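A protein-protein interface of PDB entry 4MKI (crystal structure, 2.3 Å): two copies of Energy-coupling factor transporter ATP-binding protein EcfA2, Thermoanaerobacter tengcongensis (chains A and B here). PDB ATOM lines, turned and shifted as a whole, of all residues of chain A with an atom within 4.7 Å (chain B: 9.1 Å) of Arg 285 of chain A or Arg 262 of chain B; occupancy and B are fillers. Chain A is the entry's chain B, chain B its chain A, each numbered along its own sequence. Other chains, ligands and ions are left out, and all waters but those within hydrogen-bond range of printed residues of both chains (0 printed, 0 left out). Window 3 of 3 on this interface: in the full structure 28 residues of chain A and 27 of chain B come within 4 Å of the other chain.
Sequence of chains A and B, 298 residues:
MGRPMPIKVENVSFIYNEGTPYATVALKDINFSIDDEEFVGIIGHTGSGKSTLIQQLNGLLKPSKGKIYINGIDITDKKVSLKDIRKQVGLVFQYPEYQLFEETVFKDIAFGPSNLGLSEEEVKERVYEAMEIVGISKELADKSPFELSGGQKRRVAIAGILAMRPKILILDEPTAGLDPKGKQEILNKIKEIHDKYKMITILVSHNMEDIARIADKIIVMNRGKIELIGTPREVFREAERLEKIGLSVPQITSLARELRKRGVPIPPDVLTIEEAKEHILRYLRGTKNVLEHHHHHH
Tyr 283 of chain A touches Leu 284 of chain B, and with the chains exchanged Leu 284 of chain A touches Tyr 283 of chain B. Leu 284 of chain B touches its own counterpart, Leu 284 of chain A. Positions printed for both chains: 283 and 284. Of the 8 pairs that touch across the chains among the printed residues, 3 have their exchanged pair printed and touching as well.
The guanidinium group (NH1) of Arg 262 of chain B sits close to the guanidinium group (NH2) of Arg 285 of chain A, at 3.1 Å.
Leu 259 of chain B touches Leu 281 of chain A. Leu 281 of chain A touches Arg 262 of chain B. Val 264 of chain B touches Leu 281 of chain A (CG2 to CD2, 3.99 Å). Tyr 283 of chain A touches Leu 284 of chain B (CE2 to CD2, 3.96 Å). Val 264 of chain B touches Leu 284 of chain A (CG2 to CD1, 3.9 Å). Leu 284 of chain A touches Tyr 283 of chain B. Leu 284 of chain A touches Leu 284 of chain B.
Arg 285 of chain A touches just one residue of chain B: Arg 262. Arg 262 of chain B touches two residues of chain A. Printed residues of chain B within 4 Å of Leu 281 of chain A: Leu 259, Arg 262 and Val 264. Printed residues of chain A within 4 Å of Val 264 of chain B: Leu 281 and Leu 284. Leu 255 of chain B touches none of the printed residues of chain A. Thr 287 of chain A touches none of the printed residues of chain B. The nearest printed residue of chain A that does not touch Tyr 283 of chain B is Leu 281 of chain A (7.9 Å).
The backbone NH (N) of Val 264 of chain B is in hydrogen-bond range of the backbone carbonyl oxygen (O) of Leu 259 of chain B (3.0 Å).
Along chain A the printed residues that touch a printed residue of chain B span positions 281 to 285. Of the 14 printed residues of chain B, 5 touch a printed residue of chain A. Printed residues of chain B that touch a printed residue of chain A: Leu 259, Arg 262, Val 264, Tyr 283 and Leu 284. Among the printed residues, 8 pairs touch across the chains.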
ATOM      1  N   LEU A 281     -29.583 -26.366  -6.994  1.00  0.00           N
ATOM      2  CA  LEU A 281     -28.500 -25.509  -7.497  1.00  0.00           C
ATOM      3  C   LEU A 281     -27.861 -24.732  -6.361  1.00  0.00           C
ATOM      4  O   LEU A 281     -26.672 -24.515  -6.370  1.00  0.00           O
ATOM      5  CB  LEU A 281     -28.995 -24.535  -8.579  1.00  0.00           C
ATOM      6  CG  LEU A 281     -29.496 -25.211  -9.855  1.00  0.00           C
ATOM      7  CD1 LEU A 281     -29.945 -24.200 -10.897  1.00  0.00           C
ATOM      8  CD2 LEU A 281     -28.441 -26.152 -10.399  1.00  0.00           C
ATOM      9  N   ARG A 282     -28.661 -24.311  -5.392  1.00  0.00           N
ATOM     10  CA  ARG A 282     -28.136 -23.622  -4.234  1.00  0.00           C
ATOM     11  C   ARG A 282     -27.153 -24.490  -3.466  1.00  0.00           C
ATOM     12  O   ARG A 282     -26.151 -23.984  -2.990  1.00  0.00           O
ATOM     13  CB  ARG A 282     -29.273 -23.227  -3.302  1.00  0.00           C
ATOM     14  CG  ARG A 282     -29.182 -21.839  -2.675  1.00  0.00           C
ATOM     15  CD  ARG A 282     -30.314 -20.942  -3.159  1.00  0.00           C
ATOM     16  NE  ARG A 282     -31.545 -21.119  -2.398  1.00  0.00           N
ATOM     17  CZ  ARG A 282     -32.760 -20.849  -2.870  1.00  0.00           C
ATOM     18  NH1 ARG A 282     -32.940 -20.403  -4.120  1.00  0.00           N
ATOM     19  NH2 ARG A 282     -33.809 -21.028  -2.086  1.00  0.00           N
ATOM     20  N   TYR A 283     -27.440 -25.774  -3.306  1.00  0.00           N
ATOM     21  CA  TYR A 283     -26.511 -26.650  -2.572  1.00  0.00           C
ATOM     22  C   TYR A 283     -25.179 -26.804  -3.315  1.00  0.00           C
ATOM     23  O   TYR A 283     -24.122 -26.931  -2.704  1.00  0.00           O
ATOM     24  CB  TYR A 283     -27.142 -28.002  -2.319  1.00  0.00           C
ATOM     25  CG  TYR A 283     -26.305 -29.021  -1.567  1.00  0.00           C
ATOM     26  CD1 TYR A 283     -25.712 -28.709  -0.350  1.00  0.00           C
ATOM     27  CD2 TYR A 283     -26.172 -30.327  -2.034  1.00  0.00           C
ATOM     28  CE1 TYR A 283     -24.969 -29.656   0.354  1.00  0.00           C
ATOM     29  CE2 TYR A 283     -25.437 -31.281  -1.331  1.00  0.00           C
ATOM     30  CZ  TYR A 283     -24.838 -30.939  -0.145  1.00  0.00           C
ATOM     31  OH  TYR A 283     -24.146 -31.878   0.568  1.00  0.00           O
ATOM     32  N   LEU A 284     -25.238 -26.767  -4.637  1.00  0.00           N
ATOM     33  CA  LEU A 284     -24.040 -26.862  -5.467  1.00  0.00           C
ATOM     34  C   LEU A 284     -23.221 -25.574  -5.452  1.00  0.00           C
ATOM     35  O   LEU A 284     -22.028 -25.628  -5.255  1.00  0.00           O
ATOM     36  CB  LEU A 284     -24.418 -27.253  -6.893  1.00  0.00           C
ATOM     37  CG  LEU A 284     -24.940 -28.686  -6.992  1.00  0.00           C
ATOM     38  CD1 LEU A 284     -25.603 -28.922  -8.338  1.00  0.00           C
ATOM     39  CD2 LEU A 284     -23.799 -29.656  -6.746  1.00  0.00           C
ATOM     40  N   ARG A 285     -23.862 -24.426  -5.631  1.00  0.00           N
ATOM     41  CA  ARG A 285     -23.177 -23.132  -5.457  1.00  0.00           C
ATOM     42  C   ARG A 285     -22.792 -22.842  -3.983  1.00  0.00           C
ATOM     43  O   ARG A 285     -21.976 -21.968  -3.736  1.00  0.00           O
ATOM     44  CB  ARG A 285     -24.003 -21.975  -6.058  1.00  0.00           C
ATOM     45  CG  ARG A 285     -23.806 -21.823  -7.586  1.00  0.00           C
ATOM     46  CD  ARG A 285     -25.061 -22.154  -8.402  1.00  0.00           C
ATOM     47  NE  ARG A 285     -25.903 -20.973  -8.634  1.00  0.00           N
ATOM     48  CZ  ARG A 285     -26.456 -20.646  -9.807  1.00  0.00           C
ATOM     49  NH1 ARG A 285     -27.186 -19.539  -9.898  1.00  0.00           N
ATOM     50  NH2 ARG A 285     -26.302 -21.409 -10.890  1.00  0.00           N
ATOM     51  N   GLY A 286     -23.331 -23.607  -3.027  1.00  0.00           N
ATOM     52  CA  GLY A 286     -23.143 -23.363  -1.593  1.00  0.00           C
ATOM     53  C   GLY A 286     -21.901 -24.074  -1.062  1.00  0.00           C
ATOM     54  O   GLY A 286     -21.119 -23.496  -0.297  1.00  0.00           O
ATOM     55  N   THR A 287     -21.733 -25.342  -1.444  1.00  0.00           N
ATOM     56  CA  THR A 287     -20.424 -25.999  -1.370  1.00  0.00           C
ATOM     57  C   THR A 287     -19.833 -25.907  -2.794  1.00  0.00           C
ATOM     58  O   THR A 287     -18.747 -26.423  -3.089  1.00  0.00           O
ATOM     59  CB  THR A 287     -20.511 -27.453  -0.818  1.00  0.00           C
ATOM     60  OG1 THR A 287     -20.894 -28.370  -1.850  1.00  0.00           O
ATOM     61  CG2 THR A 287     -21.513 -27.548   0.343  1.00  0.00           C
ATOM     62  N   LEU B 255     -37.350 -31.825 -14.648  1.00  0.00           N
ATOM     63  CA  LEU B 255     -36.347 -31.385 -13.672  1.00  0.00           C
ATOM     64  C   LEU B 255     -34.917 -31.731 -14.148  1.00  0.00           C
ATOM     65  O   LEU B 255     -34.067 -30.887 -14.167  1.00  0.00           O
ATOM     66  CB  LEU B 255     -36.661 -32.021 -12.308  1.00  0.00           C
ATOM     67  CG  LEU B 255     -35.922 -31.611 -11.037  1.00  0.00           C
ATOM     68  CD1 LEU B 255     -34.822 -32.593 -10.734  1.00  0.00           C
ATOM     69  CD2 LEU B 255     -35.369 -30.195 -11.096  1.00  0.00           C
ATOM     70  N   ALA B 256     -34.679 -32.980 -14.546  1.00  0.00           N
ATOM     71  CA  ALA B 256     -33.348 -33.427 -15.004  1.00  0.00           C
ATOM     72  C   ALA B 256     -32.872 -32.558 -16.167  1.00  0.00           C
ATOM     73  O   ALA B 256     -31.734 -32.156 -16.232  1.00  0.00           O
ATOM     74  CB  ALA B 256     -33.408 -34.883 -15.432  1.00  0.00           C
ATOM     75  N   ARG B 257     -33.803 -32.238 -17.045  1.00  0.00           N
ATOM     76  CA  ARG B 257     -33.610 -31.352 -18.152  1.00  0.00           C
ATOM     77  C   ARG B 257     -33.195 -29.964 -17.690  1.00  0.00           C
ATOM     78  O   ARG B 257     -32.271 -29.355 -18.240  1.00  0.00           O
ATOM     79  CB  ARG B 257     -34.962 -31.220 -18.828  1.00  0.00           C
ATOM     80  CG  ARG B 257     -34.963 -30.623 -20.211  1.00  0.00           C
ATOM     81  CD  ARG B 257     -34.897 -31.741 -21.207  1.00  0.00           C
ATOM     82  NE  ARG B 257     -35.126 -31.221 -22.538  1.00  0.00           N
ATOM     83  CZ  ARG B 257     -34.778 -31.847 -23.651  1.00  0.00           C
ATOM     84  NH1 ARG B 257     -34.185 -33.044 -23.604  1.00  0.00           N
ATOM     85  NH2 ARG B 257     -35.050 -31.277 -24.827  1.00  0.00           N
ATOM     86  N   GLU B 258     -33.917 -29.436 -16.708  1.00  0.00           N
ATOM     87  CA  GLU B 258     -33.653 -28.093 -16.204  1.00  0.00           C
ATOM     88  C   GLU B 258     -32.328 -27.988 -15.454  1.00  0.00           C
ATOM     89  O   GLU B 258     -31.694 -26.950 -15.482  1.00  0.00           O
ATOM     90  CB  GLU B 258     -34.800 -27.613 -15.321  1.00  0.00           C
ATOM     91  CG  GLU B 258     -36.019 -27.209 -16.118  1.00  0.00           C
ATOM     92  CD  GLU B 258     -35.867 -25.828 -16.710  1.00  0.00           C
ATOM     93  OE1 GLU B 258     -35.888 -24.837 -15.937  1.00  0.00           O
ATOM     94  OE2 GLU B 258     -35.716 -25.739 -17.945  1.00  0.00           O
ATOM     95  N   LEU B 259     -31.926 -29.068 -14.783  1.00  0.00           N
ATOM     96  CA  LEU B 259     -30.645 -29.121 -14.092  1.00  0.00           C
ATOM     97  C   LEU B 259     -29.511 -29.233 -15.100  1.00  0.00           C
ATOM     98  O   LEU B 259     -28.475 -28.602 -14.930  1.00  0.00           O
ATOM     99  CB  LEU B 259     -30.577 -30.316 -13.143  1.00  0.00           C
ATOM    100  CG  LEU B 259     -31.475 -30.251 -11.902  1.00  0.00           C
ATOM    101  CD1 LEU B 259     -31.438 -31.552 -11.159  1.00  0.00           C
ATOM    102  CD2 LEU B 259     -31.029 -29.137 -10.982  1.00  0.00           C
ATOM    103  N   ARG B 260     -29.710 -30.011 -16.158  1.00  0.00           N
ATOM    104  CA  ARG B 260     -28.728 -30.085 -17.237  1.00  0.00           C
ATOM    105  C   ARG B 260     -28.476 -28.711 -17.877  1.00  0.00           C
ATOM    106  O   ARG B 260     -27.332 -28.288 -17.991  1.00  0.00           O
ATOM    107  CB  ARG B 260     -29.170 -31.093 -18.296  1.00  0.00           C
ATOM    108  CG  ARG B 260     -28.085 -32.052 -18.665  1.00  0.00           C
ATOM    109  CD  ARG B 260     -28.319 -32.578 -20.051  1.00  0.00           C
ATOM    110  NE  ARG B 260     -27.419 -33.683 -20.410  1.00  0.00           N
ATOM    111  CZ  ARG B 260     -27.270 -34.125 -21.660  1.00  0.00           C
ATOM    112  NH1 ARG B 260     -27.938 -33.538 -22.669  1.00  0.00           N
ATOM    113  NH2 ARG B 260     -26.449 -35.148 -21.924  1.00  0.00           N
ATOM    114  N   LYS B 261     -29.532 -28.003 -18.262  1.00  0.00           N
ATOM    115  CA  LYS B 261     -29.373 -26.659 -18.835  1.00  0.00           C
ATOM    116  C   LYS B 261     -28.465 -25.779 -17.973  1.00  0.00           C
ATOM    117  O   LYS B 261     -27.611 -25.086 -18.490  1.00  0.00           O
ATOM    118  CB  LYS B 261     -30.718 -25.944 -19.007  1.00  0.00           C
ATOM    119  CG  LYS B 261     -31.651 -26.514 -20.073  1.00  0.00           C
ATOM    120  CD  LYS B 261     -33.079 -25.978 -19.972  1.00  0.00           C
ATOM    121  CE  LYS B 261     -33.191 -24.439 -19.883  1.00  0.00           C
ATOM    122  NZ  LYS B 261     -33.918 -23.856 -21.058  1.00  0.00           N
ATOM    123  N   ARG B 262     -28.638 -25.835 -16.659  1.00  0.00           N
ATOM    124  CA  ARG B 262     -27.879 -24.984 -15.769  1.00  0.00           C
ATOM    125  C   ARG B 262     -26.487 -25.520 -15.400  1.00  0.00           C
ATOM    126  O   ARG B 262     -25.853 -24.955 -14.531  1.00  0.00           O
ATOM    127  CB  ARG B 262     -28.685 -24.731 -14.496  1.00  0.00           C
ATOM    128  CG  ARG B 262     -30.013 -24.033 -14.751  1.00  0.00           C
ATOM    129  CD  ARG B 262     -29.856 -22.567 -15.136  1.00  0.00           C
ATOM    130  NE  ARG B 262     -30.591 -21.706 -14.197  1.00  0.00           N
ATOM    131  CZ  ARG B 262     -30.125 -21.281 -13.019  1.00  0.00           C
ATOM    132  NH1 ARG B 262     -28.898 -21.609 -12.611  1.00  0.00           N
ATOM    133  NH2 ARG B 262     -30.894 -20.519 -12.244  1.00  0.00           N
ATOM    134  N   GLY B 263     -26.022 -26.598 -16.022  1.00  0.00           N
ATOM    135  CA  GLY B 263     -24.687 -27.124 -15.745  1.00  0.00           C
ATOM    136  C   GLY B 263     -24.524 -28.524 -15.162  1.00  0.00           C
ATOM    137  O   GLY B 263     -23.446 -29.101 -15.239  1.00  0.00           O
ATOM    138  N   VAL B 264     -25.570 -29.094 -14.585  1.00  0.00           N
ATOM    139  CA  VAL B 264     -25.426 -30.371 -13.898  1.00  0.00           C
ATOM    140  C   VAL B 264     -25.373 -31.546 -14.903  1.00  0.00           C
ATOM    141  O   VAL B 264     -26.229 -31.640 -15.776  1.00  0.00           O
ATOM    142  CB  VAL B 264     -26.567 -30.599 -12.882  1.00  0.00           C
ATOM    143  CG1 VAL B 264     -26.289 -31.815 -12.013  1.00  0.00           C
ATOM    144  CG2 VAL B 264     -26.744 -29.388 -11.996  1.00  0.00           C
ATOM    145  N   PRO B 265     -24.378 -32.447 -14.771  1.00  0.00           N
ATOM    146  CA  PRO B 265     -24.225 -33.610 -15.660  1.00  0.00           C
ATOM    147  C   PRO B 265     -25.136 -34.801 -15.336  1.00  0.00           C
ATOM    148  O   PRO B 265     -24.667 -35.908 -15.048  1.00  0.00           O
ATOM    149  CB  PRO B 265     -22.743 -33.999 -15.518  1.00  0.00           C
ATOM    150  CG  PRO B 265     -22.280 -33.374 -14.254  1.00  0.00           C
ATOM    151  CD  PRO B 265     -23.241 -32.289 -13.846  1.00  0.00           C
ATOM    152  N   ILE B 266     -26.435 -34.570 -15.442  1.00  0.00           N
ATOM    153  CA  ILE B 266     -27.474 -35.583 -15.239  1.00  0.00           C
ATOM    154  C   ILE B 266     -27.980 -35.962 -16.625  1.00  0.00           C
ATOM    155  O   ILE B 266     -28.163 -35.083 -17.462  1.00  0.00           O
ATOM    156  CB  ILE B 266     -28.715 -35.009 -14.503  1.00  0.00           C
ATOM    157  CG1 ILE B 266     -28.289 -34.106 -13.367  1.00  0.00           C
ATOM    158  CG2 ILE B 266     -29.624 -36.126 -13.998  1.00  0.00           C
ATOM    159  CD1 ILE B 266     -29.452 -33.609 -12.553  1.00  0.00           C
ATOM    160  N   TYR B 283     -23.672 -37.915  -8.435  1.00  0.00           N
ATOM    161  CA  TYR B 283     -22.973 -36.738  -8.884  1.00  0.00           C
ATOM    162  C   TYR B 283     -22.437 -35.926  -7.704  1.00  0.00           C
ATOM    163  O   TYR B 283     -21.374 -35.312  -7.792  1.00  0.00           O
ATOM    164  CB  TYR B 283     -23.903 -35.875  -9.724  1.00  0.00           C
ATOM    165  CG  TYR B 283     -23.324 -34.491  -9.943  1.00  0.00           C
ATOM    166  CD1 TYR B 283     -22.161 -34.298 -10.719  1.00  0.00           C
ATOM    167  CD2 TYR B 283     -23.862 -33.387  -9.308  1.00  0.00           C
ATOM    168  CE1 TYR B 283     -21.616 -33.035 -10.898  1.00  0.00           C
ATOM    169  CE2 TYR B 283     -23.315 -32.120  -9.495  1.00  0.00           C
ATOM    170  CZ  TYR B 283     -22.197 -31.964 -10.289  1.00  0.00           C
ATOM    171  OH  TYR B 283     -21.653 -30.728 -10.466  1.00  0.00           O
ATOM    172  N   LEU B 284     -23.193 -35.886  -6.610  1.00  0.00           N
ATOM    173  CA  LEU B 284     -22.753 -35.169  -5.422  1.00  0.00           C
ATOM    174  C   LEU B 284     -21.608 -35.884  -4.756  1.00  0.00           C
ATOM    175  O   LEU B 284     -20.604 -35.279  -4.427  1.00  0.00           O
ATOM    176  CB  LEU B 284     -23.902 -35.000  -4.447  1.00  0.00           C
ATOM    177  CG  LEU B 284     -24.972 -34.022  -4.915  1.00  0.00           C
ATOM    178  CD1 LEU B 284     -26.226 -34.116  -4.026  1.00  0.00           C
ATOM    179  CD2 LEU B 284     -24.386 -32.625  -4.905  1.00  0.00           C
